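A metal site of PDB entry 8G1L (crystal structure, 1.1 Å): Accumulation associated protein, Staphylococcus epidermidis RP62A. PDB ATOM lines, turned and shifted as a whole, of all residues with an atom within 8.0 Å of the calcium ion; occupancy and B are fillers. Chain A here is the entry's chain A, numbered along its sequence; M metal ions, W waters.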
ATOM      1  N   ASN A  73      10.448  20.310  -1.124  1.00  0.00           N
ATOM      2  CA  ASN A  73      11.755  20.388  -1.753  1.00  0.00           C
ATOM      3  C   ASN A  73      11.735  21.110  -3.092  1.00  0.00           C
ATOM      4  O   ASN A  73      12.798  21.340  -3.662  1.00  0.00           O
ATOM      5  CB  ASN A  73      12.444  19.037  -1.812  1.00  0.00           C
ATOM      6  CG  ASN A  73      11.834  18.067  -2.787  1.00  0.00           C
ATOM      7  OD1 ASN A  73      11.077  18.440  -3.687  1.00  0.00           O
ATOM      8  ND2 ASN A  73      12.232  16.810  -2.654  1.00  0.00           N
ATOM      9  N   ALA A  77      14.788  25.801   0.477  1.00  0.00           N
ATOM     10  CA  ALA A  77      16.206  25.953   0.205  1.00  0.00           C
ATOM     11  C   ALA A  77      16.835  24.663  -0.325  1.00  0.00           C
ATOM     12  O   ALA A  77      16.256  23.575  -0.261  1.00  0.00           O
ATOM     13  CB  ALA A  77      16.913  26.365   1.493  1.00  0.00           C
ATOM     14  N   ASP A  78      18.077  24.814  -0.799  1.00  0.00           N
ATOM     15  CA  ASP A  78      18.812  23.686  -1.376  1.00  0.00           C
ATOM     16  C   ASP A  78      19.337  22.730  -0.319  1.00  0.00           C
ATOM     17  O   ASP A  78      19.492  21.528  -0.590  1.00  0.00           O
ATOM     18  CB  ASP A  78      19.969  24.239  -2.220  1.00  0.00           C
ATOM     19  CG  ASP A  78      19.517  25.183  -3.314  1.00  0.00           C
ATOM     20  OD1 ASP A  78      18.374  25.028  -3.780  1.00  0.00           O
ATOM     21  OD2 ASP A  78      20.310  26.072  -3.685  1.00  0.00           O
ATOM     22  N   GLY A  79      19.644  23.237   0.881  1.00  0.00           N
ATOM     23  CA  GLY A  79      20.139  22.436   1.983  1.00  0.00           C
ATOM     24  C   GLY A  79      21.253  23.126   2.722  1.00  0.00           C
ATOM     25  O   GLY A  79      21.348  24.360   2.721  1.00  0.00           O
ATOM     26  N   ILE A  98      28.654  22.693  -2.470  1.00  0.00           N
ATOM     27  CA  ILE A  98      28.532  21.238  -2.484  1.00  0.00           C
ATOM     28  C   ILE A  98      27.076  20.773  -2.428  1.00  0.00           C
ATOM     29  O   ILE A  98      26.819  19.624  -2.057  1.00  0.00           O
ATOM     30  CB  ILE A  98      29.399  20.590  -1.382  1.00  0.00           C
ATOM     31  CG1 ILE A  98      29.068  21.131   0.010  1.00  0.00           C
ATOM     32  CG2 ILE A  98      30.871  20.741  -1.710  1.00  0.00           C
ATOM     33  CD1 ILE A  98      29.653  20.304   1.125  1.00  0.00           C
ATOM     34  N   LEU A  99      26.136  21.640  -2.828  1.00  0.00           N
ATOM     35  CA  LEU A  99      24.712  21.359  -2.781  1.00  0.00           C
ATOM     36  C   LEU A  99      24.081  21.120  -4.147  1.00  0.00           C
ATOM     37  O   LEU A  99      22.864  20.894  -4.232  1.00  0.00           O
ATOM     38  CB  LEU A  99      23.965  22.481  -2.044  1.00  0.00           C
ATOM     39  CG  LEU A  99      23.991  22.366  -0.523  1.00  0.00           C
ATOM     40  CD1 LEU A  99      23.643  23.671   0.128  1.00  0.00           C
ATOM     41  CD2 LEU A  99      23.053  21.261  -0.083  1.00  0.00           C
ATOM     42  N   ARG A 100      24.881  21.141  -5.219  1.00  0.00           N
ATOM     43  CA  ARG A 100      24.396  21.022  -6.594  1.00  0.00           C
ATOM     44  C   ARG A 100      25.257  19.997  -7.323  1.00  0.00           C
ATOM     45  O   ARG A 100      25.843  19.099  -6.719  1.00  0.00           O
ATOM     46  CB  ARG A 100      24.357  22.429  -7.221  1.00  0.00           C
ATOM     47  CG  ARG A 100      23.204  23.260  -6.752  1.00  0.00           C
ATOM     48  CD  ARG A 100      21.946  22.704  -7.407  1.00  0.00           C
ATOM     49  NE  ARG A 100      20.685  23.376  -7.123  1.00  0.00           N
ATOM     50  CZ  ARG A 100      20.136  24.331  -7.870  1.00  0.00           C
ATOM     51  NH1 ARG A 100      20.742  24.813  -8.949  1.00  0.00           N
ATOM     52  NH2 ARG A 100      18.980  24.800  -7.509  1.00  0.00           N
ATOM     53  N   GLU A 101      25.308  20.118  -8.657  1.00  0.00           N
ATOM     54  CA  GLU A 101      26.062  19.210  -9.513  1.00  0.00           C
ATOM     55  C   GLU A 101      27.488  19.700  -9.740  1.00  0.00           C
ATOM     56  O   GLU A 101      28.337  18.910 -10.205  1.00  0.00           O
ATOM     57  CB  GLU A 101      25.335  19.044 -10.858  1.00  0.00           C
ATOM     58  CG  GLU A 101      25.611  20.082 -11.954  1.00  0.00           C
ATOM     59  CD  GLU A 101      24.991  21.465 -11.757  1.00  0.00           C
ATOM     60  OE1 GLU A 101      24.415  21.760 -10.689  1.00  0.00           O
ATOM     61  OE2 GLU A 101      25.060  22.267 -12.729  1.00  0.00           O
ATOM     62  N   ARG A 111      26.921  17.150   3.010  1.00  0.00           N
ATOM     63  CA  ARG A 111      25.755  17.717   2.344  1.00  0.00           C
ATOM     64  C   ARG A 111      24.479  17.205   3.001  1.00  0.00           C
ATOM     65  O   ARG A 111      24.249  15.999   3.046  1.00  0.00           O
ATOM     66  CB  ARG A 111      25.786  17.277   0.871  1.00  0.00           C
ATOM     67  CG  ARG A 111      24.661  17.770  -0.032  1.00  0.00           C
ATOM     68  CD  ARG A 111      24.774  17.099  -1.361  1.00  0.00           C
ATOM     69  NE  ARG A 111      23.823  17.344  -2.408  1.00  0.00           N
ATOM     70  CZ  ARG A 111      24.151  17.636  -3.666  1.00  0.00           C
ATOM     71  NH1 ARG A 111      23.220  17.570  -4.612  1.00  0.00           N
ATOM     72  NH2 ARG A 111      25.378  18.042  -3.985  1.00  0.00           N
ATOM     73  N   ILE A 112      23.668  18.131   3.533  1.00  0.00           N
ATOM     74  CA  ILE A 112      22.298  17.838   3.944  1.00  0.00           C
ATOM     75  C   ILE A 112      21.410  18.451   2.878  1.00  0.00           C
ATOM     76  O   ILE A 112      21.258  19.675   2.819  1.00  0.00           O
ATOM     77  CB  ILE A 112      21.947  18.357   5.342  1.00  0.00           C
ATOM     78  CG1 ILE A 112      22.873  17.786   6.416  1.00  0.00           C
ATOM     79  CG2 ILE A 112      20.487  18.017   5.653  1.00  0.00           C
ATOM     80  CD1 ILE A 112      22.669  18.395   7.803  1.00  0.00           C
ATOM     81  N   ASP A 113      20.865  17.627   2.003  1.00  0.00           N
ATOM     82  CA  ASP A 113      20.196  18.085   0.794  1.00  0.00           C
ATOM     83  C   ASP A 113      18.699  18.153   1.032  1.00  0.00           C
ATOM     84  O   ASP A 113      18.080  17.122   1.320  1.00  0.00           O
ATOM     85  CB  ASP A 113      20.531  17.139  -0.356  1.00  0.00           C
ATOM     86  CG  ASP A 113      20.128  17.697  -1.697  1.00  0.00           C
ATOM     87  OD1 ASP A 113      19.012  18.243  -1.798  1.00  0.00           O
ATOM     88  OD2 ASP A 113      20.918  17.587  -2.672  1.00  0.00           O
ATOM     89  N   THR A 114      18.130  19.356   0.933  1.00  0.00           N
ATOM     90  CA  THR A 114      16.714  19.589   1.183  1.00  0.00           C
ATOM     91  C   THR A 114      15.960  20.133  -0.023  1.00  0.00           C
ATOM     92  O   THR A 114      14.745  20.372   0.080  1.00  0.00           O
ATOM     93  CB  THR A 114      16.516  20.529   2.382  1.00  0.00           C
ATOM     94  OG1 THR A 114      17.052  21.818   2.074  1.00  0.00           O
ATOM     95  CG2 THR A 114      17.226  20.021   3.608  1.00  0.00           C
ATOM     96  N   GLY A 115      16.615  20.333  -1.167  1.00  0.00           N
ATOM     97  CA  GLY A 115      16.002  20.980  -2.312  1.00  0.00           C
ATOM     98  C   GLY A 115      16.247  20.223  -3.600  1.00  0.00           C
ATOM     99  O   GLY A 115      17.383  19.847  -3.894  1.00  0.00           O
ATOM    100  N   TYR A 116      15.192  20.004  -4.389  1.00  0.00           N
ATOM    101  CA  TYR A 116      15.292  19.264  -5.635  1.00  0.00           C
ATOM    102  C   TYR A 116      15.729  20.176  -6.783  1.00  0.00           C
ATOM    103  O   TYR A 116      15.192  21.278  -6.961  1.00  0.00           O
ATOM    104  CB  TYR A 116      13.922  18.660  -5.960  1.00  0.00           C
ATOM    105  CG  TYR A 116      13.947  17.943  -7.279  1.00  0.00           C
ATOM    106  CD1 TYR A 116      14.552  16.701  -7.383  1.00  0.00           C
ATOM    107  CD2 TYR A 116      13.430  18.507  -8.446  1.00  0.00           C
ATOM    108  CE1 TYR A 116      14.635  16.036  -8.582  1.00  0.00           C
ATOM    109  CE2 TYR A 116      13.513  17.843  -9.656  1.00  0.00           C
ATOM    110  CZ  TYR A 116      14.116  16.598  -9.720  1.00  0.00           C
ATOM    111  OH  TYR A 116      14.230  15.915 -10.919  1.00  0.00           O
ATOM    112  N   TYR A 117      16.686  19.706  -7.571  1.00  0.00           N
ATOM    113  CA  TYR A 117      17.129  20.393  -8.782  1.00  0.00           C
ATOM    114  C   TYR A 117      17.055  19.413  -9.943  1.00  0.00           C
ATOM    115  O   TYR A 117      17.671  18.349  -9.897  1.00  0.00           O
ATOM    116  CB  TYR A 117      18.543  20.944  -8.610  1.00  0.00           C
ATOM    117  CG  TYR A 117      19.108  21.640  -9.842  1.00  0.00           C
ATOM    118  CD1 TYR A 117      18.354  22.513 -10.601  1.00  0.00           C
ATOM    119  CD2 TYR A 117      20.423  21.425 -10.227  1.00  0.00           C
ATOM    120  CE1 TYR A 117      18.895  23.147 -11.720  1.00  0.00           C
ATOM    121  CE2 TYR A 117      20.972  22.068 -11.334  1.00  0.00           C
ATOM    122  CZ  TYR A 117      20.207  22.928 -12.076  1.00  0.00           C
ATOM    123  OH  TYR A 117      20.748  23.562 -13.194  1.00  0.00           O
ATOM    124  N   ASN A 118      16.329  19.792 -10.991  1.00  0.00           N
ATOM    125  CA  ASN A 118      16.046  18.853 -12.072  1.00  0.00           C
ATOM    126  C   ASN A 118      17.290  18.471 -12.872  1.00  0.00           C
ATOM    127  O   ASN A 118      17.245  17.471 -13.590  1.00  0.00           O
ATOM    128  CB  ASN A 118      14.949  19.397 -12.978  1.00  0.00           C
ATOM    129  CG  ASN A 118      14.189  18.285 -13.716  1.00  0.00           C
ATOM    130  OD1 ASN A 118      13.725  17.314 -13.119  1.00  0.00           O
ATOM    131  ND2 ASN A 118      14.096  18.436 -15.026  1.00  0.00           N
ATOM    132  N   ASP A 120      20.361  17.876 -11.454  1.00  0.00           N
ATOM    133  CA  ASP A 120      21.349  17.315 -10.557  1.00  0.00           C
ATOM    134  C   ASP A 120      21.292  15.797 -10.602  1.00  0.00           C
ATOM    135  O   ASP A 120      20.305  15.198 -10.125  1.00  0.00           O
ATOM    136  CB  ASP A 120      21.127  17.808  -9.122  1.00  0.00           C
ATOM    137  CG  ASP A 120      22.263  17.466  -8.203  1.00  0.00           C
ATOM    138  OD1 ASP A 120      22.867  16.373  -8.393  1.00  0.00           O
ATOM    139  OD2 ASP A 120      22.565  18.272  -7.296  1.00  0.00           O
ATOM    140  N   LEU A 122      22.730  13.562  -8.866  1.00  0.00           N
ATOM    141  CA  LEU A 122      22.666  12.938  -7.543  1.00  0.00           C
ATOM    142  C   LEU A 122      21.247  13.000  -6.988  1.00  0.00           C
ATOM    143  O   LEU A 122      20.788  12.045  -6.339  1.00  0.00           O
ATOM    144  CB  LEU A 122      23.667  13.581  -6.594  1.00  0.00           C
ATOM    145  CG  LEU A 122      23.865  12.899  -5.239  1.00  0.00           C
ATOM    146  CD1 LEU A 122      24.284  11.448  -5.376  1.00  0.00           C
ATOM    147  CD2 LEU A 122      24.890  13.668  -4.427  1.00  0.00           C
ATOM    148  N   ASP A 123      20.523  14.097  -7.229  1.00  0.00           N
ATOM    149  CA  ASP A 123      19.132  14.151  -6.784  1.00  0.00           C
ATOM    150  C   ASP A 123      18.314  13.036  -7.415  1.00  0.00           C
ATOM    151  O   ASP A 123      17.383  12.507  -6.796  1.00  0.00           O
ATOM    152  CB  ASP A 123      18.504  15.507  -7.144  1.00  0.00           C
ATOM    153  CG  ASP A 123      18.981  16.648  -6.262  1.00  0.00           C
ATOM    154  OD1 ASP A 123      19.885  16.451  -5.424  1.00  0.00           O
ATOM    155  OD2 ASP A 123      18.442  17.769  -6.428  1.00  0.00           O
ATOM    156  N   LYS A 124      18.626  12.661  -8.660  1.00  0.00           N
ATOM    157  CA  LYS A 124      17.940  11.556  -9.321  1.00  0.00           C
ATOM    158  C   LYS A 124      18.305  10.218  -8.676  1.00  0.00           C
ATOM    159  O   LYS A 124      17.432   9.411  -8.372  1.00  0.00           O
ATOM    160  CB  LYS A 124      18.220  11.578 -10.831  1.00  0.00           C
ATOM    161  N   GLN A 126      19.258   9.683  -5.663  1.00  0.00           N
ATOM    162  CA  GLN A 126      18.778   9.643  -4.289  1.00  0.00           C
ATOM    163  C   GLN A 126      17.255   9.653  -4.200  1.00  0.00           C
ATOM    164  O   GLN A 126      16.702   9.655  -3.099  1.00  0.00           O
ATOM    165  CB  GLN A 126      19.330  10.839  -3.507  1.00  0.00           C
ATOM    166  CG  GLN A 126      20.849  10.916  -3.467  1.00  0.00           C
ATOM    167  CD  GLN A 126      21.501   9.810  -2.647  1.00  0.00           C
ATOM    168  OE1 GLN A 126      21.335   8.621  -2.949  1.00  0.00           O
ATOM    169  NE2 GLN A 126      22.259  10.190  -1.631  1.00  0.00           N
ATOM    170  N   GLN A 128      15.118  12.001  -4.835  1.00  0.00           N
ATOM    171  CA  GLN A 128      14.670  13.182  -4.102  1.00  0.00           C
ATOM    172  C   GLN A 128      13.313  13.690  -4.586  1.00  0.00           C
ATOM    173  O   GLN A 128      12.534  14.220  -3.790  1.00  0.00           O
ATOM    174  CB  GLN A 128      15.730  14.288  -4.161  1.00  0.00           C
ATOM    175  CG  GLN A 128      15.307  15.537  -3.399  1.00  0.00           C
ATOM    176  CD  GLN A 128      16.460  16.463  -3.087  1.00  0.00           C
ATOM    177  OE1 GLN A 128      17.340  16.695  -3.901  1.00  0.00           O
ATOM    178  NE2 GLN A 128      16.432  17.029  -1.884  1.00  0.00           N
ATOM    179  N   ARG A 134      11.387  15.567   1.163  1.00  0.00           N
ATOM    180  CA  ARG A 134      12.325  14.536   0.750  1.00  0.00           C
ATOM    181  C   ARG A 134      13.726  15.092   0.549  1.00  0.00           C
ATOM    182  O   ARG A 134      13.936  16.017  -0.251  1.00  0.00           O
ATOM    183  CB  ARG A 134      11.885  13.871  -0.565  1.00  0.00           C
ATOM    184  CG  ARG A 134      10.563  13.140  -0.496  1.00  0.00           C
ATOM    185  CD  ARG A 134      10.202  12.545  -1.850  1.00  0.00           C
ATOM    186  NE  ARG A 134      11.063  11.449  -2.264  1.00  0.00           N
ATOM    187  CZ  ARG A 134      10.875  10.177  -1.921  1.00  0.00           C
ATOM    188  NH1 ARG A 134      11.692   9.245  -2.392  1.00  0.00           N
ATOM    189  NH2 ARG A 134       9.890   9.837  -1.105  1.00  0.00           N
ATOM    190  N   GLY A 135      14.690  14.509   1.251  1.00  0.00           N
ATOM    191  CA  GLY A 135      16.068  14.890   1.080  1.00  0.00           C
ATOM    192  C   GLY A 135      16.998  13.737   1.410  1.00  0.00           C
ATOM    193  O   GLY A 135      16.591  12.568   1.386  1.00  0.00           O
ATOM    194  N   TYR A 136      18.257  14.070   1.670  1.00  0.00           N
ATOM    195  CA  TYR A 136      19.258  13.050   1.908  1.00  0.00           C
ATOM    196  C   TYR A 136      20.474  13.699   2.519  1.00  0.00           C
ATOM    197  O   TYR A 136      20.691  14.903   2.382  1.00  0.00           O
ATOM    198  CB  TYR A 136      19.641  12.321   0.632  1.00  0.00           C
ATOM    199  CG  TYR A 136      20.145  13.138  -0.542  1.00  0.00           C
ATOM    200  CD1 TYR A 136      19.266  13.631  -1.509  1.00  0.00           C
ATOM    201  CD2 TYR A 136      21.503  13.359  -0.729  1.00  0.00           C
ATOM    202  CE1 TYR A 136      19.734  14.301  -2.629  1.00  0.00           C
ATOM    203  CE2 TYR A 136      21.981  14.029  -1.849  1.00  0.00           C
ATOM    204  CZ  TYR A 136      21.093  14.481  -2.810  1.00  0.00           C
ATOM    205  OH  TYR A 136      21.597  15.073  -3.946  1.00  0.00           O
HETATM  206 CA    CA M   1      19.236  18.490  -4.216  1.00  0.00          CA
HETATM  207  O   HOH W   1      20.842  19.562  -5.672  1.00  0.00           O
HETATM  208  O   HOH W   2      20.231  20.635  -3.188  1.00  0.00           O
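The backbone NH (N) of Gly 115 lies within hydrogen-bond range of the backbone carbonyl oxygen (O) of Asp 78.
The guanidinium group (NE) of Arg 111 lies close to the side-chain carboxylate (OD2) of Asp 113 (2.9 Å).
O of Tyr 136 lies within hydrogen-bond range of N of Asp 113 (2.8 Å).
The guanidinium group (NH1) of Arg 111 lies close to the side-chain carboxylate (OD1) of Asp 123.
The side-chain carboxylate of Asp 123 sits close to the side-chain hydroxyl of Tyr 136.
The backbone NH (N) of Asp 123 is in hydrogen-bond range of the side-chain carboxylate (OD1) of Asp 120, 3.5 Å away.
The backbone carbonyl oxygen (O) of Gln 128 is in hydrogen-bond range of the side-chain amide nitrogen (ND2) of Asn 73.
The backbone carbonyl oxygen of Arg 134 sits at hydrogen-bond distance from the side-chain amide nitrogen of Gln 128, 3.1 Å away.
Four residues have an atom within 4 Å of the calcium ion: Asp 113, Gly 115, Asp 123 and Gln 128.
The calcium ion is bound by the backbone carbonyl oxygen (O) of Gly 115 (2.3 Å), water W1 (2.4 Å), the side-chain carboxylate (OD1) of Asp 113 (2.4 Å), the side-chain carboxylate (OD2) of Asp 113 (2.5 Å), the side-chain carboxylate (OD1) of Asp 123 (2.5 Å), the side-chain carboxylate (OD2) of Asp 123 (2.5 Å), water W2 (2.6 Å) and the side-chain amide oxygen (OE1) of Gln 128 (2.6 Å).
Water W1 lies within hydrogen-bond range of OD2 of Asp 120 (2.7 Å), O of Leu 99 (2.8 Å) and NH1 of Arg 111 (3.3 Å).
Water W2 lies within hydrogen-bond range of the backbone carbonyl oxygen (O) of Leu 99 (2.8 Å) and the backbone carbonyl oxygen (O) of Asp 78 (2.8 Å).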
